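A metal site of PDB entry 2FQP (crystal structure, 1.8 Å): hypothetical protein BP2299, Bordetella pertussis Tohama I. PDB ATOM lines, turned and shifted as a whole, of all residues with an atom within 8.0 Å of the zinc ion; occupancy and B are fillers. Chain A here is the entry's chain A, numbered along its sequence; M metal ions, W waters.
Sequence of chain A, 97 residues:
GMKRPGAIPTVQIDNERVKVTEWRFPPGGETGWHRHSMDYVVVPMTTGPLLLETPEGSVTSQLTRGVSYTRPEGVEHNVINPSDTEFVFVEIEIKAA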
ATOM      1  N   TRP A  23       2.397 -36.305 -22.161  1.00  0.00           N
ATOM      2  CA  TRP A  23       1.045 -36.408 -22.716  1.00  0.00           C
ATOM      3  C   TRP A  23       1.101 -37.236 -23.979  1.00  0.00           C
ATOM      4  O   TRP A  23       1.815 -36.909 -24.921  1.00  0.00           O
ATOM      5  CB  TRP A  23       0.470 -35.009 -23.022  1.00  0.00           C
ATOM      6  CG  TRP A  23      -0.006 -34.296 -21.801  1.00  0.00           C
ATOM      7  CD1 TRP A  23       0.700 -33.415 -21.047  1.00  0.00           C
ATOM      8  CD2 TRP A  23      -1.287 -34.422 -21.187  1.00  0.00           C
ATOM      9  NE1 TRP A  23      -0.052 -32.976 -19.995  1.00  0.00           N
ATOM     10  CE2 TRP A  23      -1.285 -33.563 -20.059  1.00  0.00           C
ATOM     11  CE3 TRP A  23      -2.430 -35.187 -21.465  1.00  0.00           C
ATOM     12  CZ2 TRP A  23      -2.398 -33.454 -19.189  1.00  0.00           C
ATOM     13  CZ3 TRP A  23      -3.547 -35.068 -20.635  1.00  0.00           C
ATOM     14  CH2 TRP A  23      -3.519 -34.185 -19.498  1.00  0.00           C
ATOM     15  N   PHE A  25      -1.038 -38.862 -27.046  1.00  0.00           N
ATOM     16  CA  PHE A  25      -2.294 -38.765 -27.771  1.00  0.00           C
ATOM     17  C   PHE A  25      -2.491 -39.932 -28.682  1.00  0.00           C
ATOM     18  O   PHE A  25      -1.709 -40.131 -29.570  1.00  0.00           O
ATOM     19  CB  PHE A  25      -2.303 -37.501 -28.652  1.00  0.00           C
ATOM     20  CG  PHE A  25      -2.371 -36.219 -27.886  1.00  0.00           C
ATOM     21  CD1 PHE A  25      -1.258 -35.743 -27.161  1.00  0.00           C
ATOM     22  CD2 PHE A  25      -3.505 -35.417 -27.937  1.00  0.00           C
ATOM     23  CE1 PHE A  25      -1.309 -34.580 -26.475  1.00  0.00           C
ATOM     24  CE2 PHE A  25      -3.551 -34.203 -27.192  1.00  0.00           C
ATOM     25  CZ  PHE A  25      -2.454 -33.810 -26.465  1.00  0.00           C
ATOM     26  N   THR A  31      -7.230 -33.686 -25.366  1.00  0.00           N
ATOM     27  CA  THR A  31      -7.122 -33.417 -23.924  1.00  0.00           C
ATOM     28  C   THR A  31      -8.431 -33.232 -23.183  1.00  0.00           C
ATOM     29  O   THR A  31      -8.494 -33.512 -21.962  1.00  0.00           O
ATOM     30  CB  THR A  31      -6.293 -32.140 -23.625  1.00  0.00           C
ATOM     31  OG1 THR A  31      -6.802 -31.066 -24.421  1.00  0.00           O
ATOM     32  CG2 THR A  31      -4.846 -32.379 -23.942  1.00  0.00           C
ATOM     33  N   GLY A  32      -9.426 -32.712 -23.900  1.00  0.00           N
ATOM     34  CA  GLY A  32     -10.591 -32.065 -23.286  1.00  0.00           C
ATOM     35  C   GLY A  32     -10.202 -30.643 -22.952  1.00  0.00           C
ATOM     36  O   GLY A  32      -9.005 -30.306 -22.872  1.00  0.00           O
ATOM     37  N   TRP A  33     -11.191 -29.783 -22.793  1.00  0.00           N
ATOM     38  CA  TRP A  33     -10.914 -28.411 -22.431  1.00  0.00           C
ATOM     39  C   TRP A  33     -10.261 -28.370 -21.049  1.00  0.00           C
ATOM     40  O   TRP A  33     -10.644 -29.085 -20.152  1.00  0.00           O
ATOM     41  CB  TRP A  33     -12.206 -27.607 -22.392  1.00  0.00           C
ATOM     42  CG  TRP A  33     -11.988 -26.125 -22.489  1.00  0.00           C
ATOM     43  CD1 TRP A  33     -11.804 -25.245 -21.462  1.00  0.00           C
ATOM     44  CD2 TRP A  33     -11.950 -25.362 -23.696  1.00  0.00           C
ATOM     45  NE1 TRP A  33     -11.647 -23.969 -21.953  1.00  0.00           N
ATOM     46  CE2 TRP A  33     -11.760 -24.005 -23.318  1.00  0.00           C
ATOM     47  CE3 TRP A  33     -12.094 -25.668 -25.035  1.00  0.00           C
ATOM     48  CZ2 TRP A  33     -11.658 -22.985 -24.252  1.00  0.00           C
ATOM     49  CZ3 TRP A  33     -12.008 -24.620 -25.978  1.00  0.00           C
ATOM     50  CH2 TRP A  33     -11.787 -23.319 -25.572  1.00  0.00           C
ATOM     51  N   HIS A  34      -9.336 -27.451 -20.891  1.00  0.00           N
ATOM     52  CA  HIS A  34      -8.645 -27.210 -19.636  1.00  0.00           C
ATOM     53  C   HIS A  34      -8.083 -25.789 -19.603  1.00  0.00           C
ATOM     54  O   HIS A  34      -7.943 -25.128 -20.644  1.00  0.00           O
ATOM     55  CB  HIS A  34      -7.537 -28.261 -19.428  1.00  0.00           C
ATOM     56  CG  HIS A  34      -6.496 -28.271 -20.495  1.00  0.00           C
ATOM     57  ND1 HIS A  34      -6.729 -28.837 -21.725  1.00  0.00           N
ATOM     58  CD2 HIS A  34      -5.222 -27.779 -20.533  1.00  0.00           C
ATOM     59  CE1 HIS A  34      -5.637 -28.725 -22.466  1.00  0.00           C
ATOM     60  NE2 HIS A  34      -4.705 -28.108 -21.773  1.00  0.00           N
ATOM     61  N   ARG A  35      -7.741 -25.326 -18.399  1.00  0.00           N
ATOM     62  CA  ARG A  35      -7.128 -24.017 -18.207  1.00  0.00           C
ATOM     63  C   ARG A  35      -5.733 -24.262 -17.629  1.00  0.00           C
ATOM     64  O   ARG A  35      -5.613 -24.968 -16.644  1.00  0.00           O
ATOM     65  CB  ARG A  35      -7.917 -23.168 -17.219  1.00  0.00           C
ATOM     66  CG  ARG A  35      -7.279 -21.803 -16.959  1.00  0.00           C
ATOM     67  CD  ARG A  35      -8.106 -20.931 -15.999  1.00  0.00           C
ATOM     68  NE  ARG A  35      -7.701 -19.528 -16.086  1.00  0.00           N
ATOM     69  CZ  ARG A  35      -6.589 -19.012 -15.573  1.00  0.00           C
ATOM     70  NH1 ARG A  35      -5.726 -19.779 -14.903  1.00  0.00           N
ATOM     71  NH2 ARG A  35      -6.324 -17.705 -15.730  1.00  0.00           N
ATOM     72  N   HIS A  36      -4.713 -23.624 -18.184  1.00  0.00           N
ATOM     73  CA  HIS A  36      -3.374 -23.737 -17.635  1.00  0.00           C
ATOM     74  C   HIS A  36      -3.203 -22.787 -16.478  1.00  0.00           C
ATOM     75  O   HIS A  36      -3.289 -21.584 -16.672  1.00  0.00           O
ATOM     76  CB  HIS A  36      -2.336 -23.434 -18.687  1.00  0.00           C
ATOM     77  CG  HIS A  36      -2.152 -24.573 -19.603  1.00  0.00           C
ATOM     78  ND1 HIS A  36      -1.277 -25.604 -19.321  1.00  0.00           N
ATOM     79  CD2 HIS A  36      -2.796 -24.917 -20.749  1.00  0.00           C
ATOM     80  CE1 HIS A  36      -1.379 -26.520 -20.272  1.00  0.00           C
ATOM     81  NE2 HIS A  36      -2.292 -26.119 -21.153  1.00  0.00           N
ATOM     82  N   TYR A  40       4.150 -22.606 -18.725  1.00  0.00           N
ATOM     83  CA  TYR A  40       4.593 -23.961 -19.083  1.00  0.00           C
ATOM     84  C   TYR A  40       5.467 -24.003 -20.310  1.00  0.00           C
ATOM     85  O   TYR A  40       5.470 -23.061 -21.106  1.00  0.00           O
ATOM     86  CB  TYR A  40       3.408 -24.936 -19.174  1.00  0.00           C
ATOM     87  CG  TYR A  40       2.434 -24.689 -20.319  1.00  0.00           C
ATOM     88  CD1 TYR A  40       1.476 -23.682 -20.225  1.00  0.00           C
ATOM     89  CD2 TYR A  40       2.451 -25.483 -21.450  1.00  0.00           C
ATOM     90  CE1 TYR A  40       0.538 -23.488 -21.261  1.00  0.00           C
ATOM     91  CE2 TYR A  40       1.522 -25.278 -22.487  1.00  0.00           C
ATOM     92  CZ  TYR A  40       0.567 -24.280 -22.373  1.00  0.00           C
ATOM     93  OH  TYR A  40      -0.371 -24.026 -23.410  1.00  0.00           O
ATOM     94  N   VAL A  42       6.554 -26.646 -23.533  1.00  0.00           N
ATOM     95  CA  VAL A  42       6.198 -27.830 -24.274  1.00  0.00           C
ATOM     96  C   VAL A  42       7.454 -28.289 -25.007  1.00  0.00           C
ATOM     97  O   VAL A  42       8.028 -27.509 -25.767  1.00  0.00           O
ATOM     98  CB  VAL A  42       5.041 -27.534 -25.279  1.00  0.00           C
ATOM     99  CG1 VAL A  42       4.767 -28.725 -26.195  1.00  0.00           C
ATOM    100  CG2 VAL A  42       3.786 -27.075 -24.536  1.00  0.00           C
ATOM    101  N   LEU A  52      -5.469 -26.898 -32.305  1.00  0.00           N
ATOM    102  CA  LEU A  52      -5.719 -26.176 -31.048  1.00  0.00           C
ATOM    103  C   LEU A  52      -7.045 -25.449 -31.127  1.00  0.00           C
ATOM    104  O   LEU A  52      -7.246 -24.595 -32.009  1.00  0.00           O
ATOM    105  CB  LEU A  52      -4.602 -25.192 -30.733  1.00  0.00           C
ATOM    106  CG  LEU A  52      -3.183 -25.740 -30.773  1.00  0.00           C
ATOM    107  CD1 LEU A  52      -2.169 -24.583 -30.775  1.00  0.00           C
ATOM    108  CD2 LEU A  52      -2.980 -26.674 -29.609  1.00  0.00           C
ATOM    109  N   ARG A  71       4.282 -21.058 -23.207  1.00  0.00           N
ATOM    110  CA  ARG A  71       2.957 -20.381 -23.245  1.00  0.00           C
ATOM    111  C   ARG A  71       2.672 -19.918 -21.821  1.00  0.00           C
ATOM    112  O   ARG A  71       3.077 -20.573 -20.854  1.00  0.00           O
ATOM    113  CB  ARG A  71       1.842 -21.314 -23.701  1.00  0.00           C
ATOM    114  CG  ARG A  71       1.901 -21.828 -25.150  1.00  0.00           C
ATOM    115  CD  ARG A  71       1.877 -20.709 -26.178  1.00  0.00           C
ATOM    116  NE  ARG A  71       0.957 -19.643 -25.816  1.00  0.00           N
ATOM    117  CZ  ARG A  71      -0.382 -19.741 -25.851  1.00  0.00           C
ATOM    118  NH1 ARG A  71      -0.992 -20.858 -26.256  1.00  0.00           N
ATOM    119  NH2 ARG A  71      -1.125 -18.694 -25.470  1.00  0.00           N
ATOM    120  N   VAL A  75      -3.825 -19.878 -20.502  1.00  0.00           N
ATOM    121  CA  VAL A  75      -4.278 -20.524 -21.727  1.00  0.00           C
ATOM    122  C   VAL A  75      -5.475 -21.408 -21.437  1.00  0.00           C
ATOM    123  O   VAL A  75      -5.468 -22.184 -20.494  1.00  0.00           O
ATOM    124  CB  VAL A  75      -3.121 -21.365 -22.367  1.00  0.00           C
ATOM    125  CG1 VAL A  75      -3.630 -22.223 -23.474  1.00  0.00           C
ATOM    126  CG2 VAL A  75      -2.031 -20.410 -22.851  1.00  0.00           C
ATOM    127  N   GLU A  76      -6.520 -21.263 -22.236  1.00  0.00           N
ATOM    128  CA  GLU A  76      -7.725 -22.129 -22.167  1.00  0.00           C
ATOM    129  C   GLU A  76      -7.892 -22.713 -23.520  1.00  0.00           C
ATOM    130  O   GLU A  76      -7.976 -21.981 -24.508  1.00  0.00           O
ATOM    131  CB  GLU A  76      -8.971 -21.345 -21.790  1.00  0.00           C
ATOM    132  CG  GLU A  76      -8.942 -20.765 -20.388  1.00  0.00           C
ATOM    133  CD  GLU A  76     -10.344 -20.658 -19.741  1.00  0.00           C
ATOM    134  OE1 GLU A  76     -11.339 -21.255 -20.250  1.00  0.00           O
ATOM    135  OE2 GLU A  76     -10.406 -19.984 -18.695  1.00  0.00           O
ATOM    136  N   HIS A  77      -7.895 -24.035 -23.600  1.00  0.00           N
ATOM    137  CA  HIS A  77      -8.052 -24.709 -24.882  1.00  0.00           C
ATOM    138  C   HIS A  77      -8.326 -26.210 -24.772  1.00  0.00           C
ATOM    139  O   HIS A  77      -8.264 -26.784 -23.694  1.00  0.00           O
ATOM    140  CB  HIS A  77      -6.790 -24.506 -25.736  1.00  0.00           C
ATOM    141  CG  HIS A  77      -5.539 -25.082 -25.144  1.00  0.00           C
ATOM    142  ND1 HIS A  77      -4.303 -24.863 -25.726  1.00  0.00           N
ATOM    143  CD2 HIS A  77      -5.311 -25.839 -24.054  1.00  0.00           C
ATOM    144  CE1 HIS A  77      -3.372 -25.486 -25.033  1.00  0.00           C
ATOM    145  NE2 HIS A  77      -3.951 -26.083 -24.006  1.00  0.00           N
ATOM    146  N   ASN A  78      -8.622 -26.796 -25.926  1.00  0.00           N
ATOM    147  CA  ASN A  78      -8.710 -28.205 -26.150  1.00  0.00           C
ATOM    148  C   ASN A  78      -7.636 -28.505 -27.204  1.00  0.00           C
ATOM    149  O   ASN A  78      -7.484 -27.770 -28.157  1.00  0.00           O
ATOM    150  CB  ASN A  78     -10.076 -28.655 -26.628  1.00  0.00           C
ATOM    151  CG  ASN A  78     -10.127 -30.179 -26.902  1.00  0.00           C
ATOM    152  OD1 ASN A  78      -9.553 -30.947 -26.154  1.00  0.00           O
ATOM    153  ND2 ASN A  78     -10.778 -30.585 -28.017  1.00  0.00           N
ATOM    154  N   VAL A  79      -6.884 -29.568 -27.015  1.00  0.00           N
ATOM    155  CA  VAL A  79      -5.830 -29.880 -27.938  1.00  0.00           C
ATOM    156  C   VAL A  79      -6.101 -31.252 -28.531  1.00  0.00           C
ATOM    157  O   VAL A  79      -6.326 -32.173 -27.791  1.00  0.00           O
ATOM    158  CB  VAL A  79      -4.472 -29.979 -27.219  1.00  0.00           C
ATOM    159  CG1 VAL A  79      -3.363 -30.384 -28.175  1.00  0.00           C
ATOM    160  CG2 VAL A  79      -4.121 -28.644 -26.601  1.00  0.00           C
ATOM    161  N   PHE A  89       4.118 -35.283 -26.353  1.00  0.00           N
ATOM    162  CA  PHE A  89       4.907 -34.165 -25.869  1.00  0.00           C
ATOM    163  C   PHE A  89       5.075 -34.209 -24.355  1.00  0.00           C
ATOM    164  O   PHE A  89       4.302 -34.863 -23.645  1.00  0.00           O
ATOM    165  CB  PHE A  89       4.422 -32.770 -26.341  1.00  0.00           C
ATOM    166  CG  PHE A  89       3.053 -32.333 -25.851  1.00  0.00           C
ATOM    167  CD1 PHE A  89       2.860 -31.803 -24.554  1.00  0.00           C
ATOM    168  CD2 PHE A  89       1.970 -32.297 -26.736  1.00  0.00           C
ATOM    169  CE1 PHE A  89       1.585 -31.359 -24.151  1.00  0.00           C
ATOM    170  CE2 PHE A  89       0.724 -31.838 -26.334  1.00  0.00           C
ATOM    171  CZ  PHE A  89       0.524 -31.391 -25.046  1.00  0.00           C
ATOM    172  N   GLU A  91       5.311 -31.786 -21.121  1.00  0.00           N
ATOM    173  CA  GLU A  91       4.876 -30.490 -20.643  1.00  0.00           C
ATOM    174  C   GLU A  91       5.487 -30.212 -19.262  1.00  0.00           C
ATOM    175  O   GLU A  91       5.364 -31.013 -18.350  1.00  0.00           O
ATOM    176  CB  GLU A  91       3.334 -30.441 -20.587  1.00  0.00           C
ATOM    177  CG  GLU A  91       2.772 -29.028 -20.483  1.00  0.00           C
ATOM    178  CD  GLU A  91       1.266 -29.005 -20.880  1.00  0.00           C
ATOM    179  OE1 GLU A  91       0.433 -29.262 -20.002  1.00  0.00           O
ATOM    180  OE2 GLU A  91       0.947 -28.793 -22.066  1.00  0.00           O
ATOM    181  N   GLU A  93       5.467 -27.643 -16.265  1.00  0.00           N
ATOM    182  CA  GLU A  93       4.729 -26.533 -15.654  1.00  0.00           C
ATOM    183  C   GLU A  93       5.608 -25.974 -14.526  1.00  0.00           C
ATOM    184  O   GLU A  93       6.203 -26.728 -13.730  1.00  0.00           O
ATOM    185  CB  GLU A  93       3.377 -26.976 -15.112  1.00  0.00           C
ATOM    186  CG  GLU A  93       2.390 -27.473 -16.155  1.00  0.00           C
ATOM    187  CD  GLU A  93       1.101 -27.823 -15.497  1.00  0.00           C
ATOM    188  OE1 GLU A  93       1.021 -28.932 -14.934  1.00  0.00           O
ATOM    189  OE2 GLU A  93       0.197 -26.969 -15.474  1.00  0.00           O
HETATM  190 ZN    ZN M   1      -2.930 -27.488 -22.515  1.00  0.00          ZN
HETATM  191  O   HOH W   1      -2.971 -29.411 -23.725  1.00  0.00           O
HETATM  192  O   HOH W   2      -1.968 -29.415 -21.483  1.00  0.00           O
HETATM  193  O   HOH W   3      -1.100 -27.733 -23.377  1.00  0.00           O
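OG1 of Thr 31 lies close to ND1 of His 34 (3.5 Å). ND1 of His 34 is in hydrogen-bond range of O of Gly 32, 2.9 Å away. The backbone NH (N) of His 36 lies within hydrogen-bond range of the backbone carbonyl oxygen (O) of Val 75, 2.8 Å away.
Three residues have an atom within 4 Å of the zinc ion: His 34, His 36 and His 77. Along chain A the residues within 4 Å of the zinc ion span positions 34 to 77. The nearest printed residue that does not touch the zinc ion is Glu 91 (4.1 Å).
The zinc ion is bound by NE2 of His 34 (2.0 Å), NE2 of His 36 (2.0 Å), water W3 (2.0 Å), water W1 (2.3 Å), NE2 of His 77 (2.3 Å) and water W2 (2.4 Å). The zinc ion has six donor atoms within binding distance.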
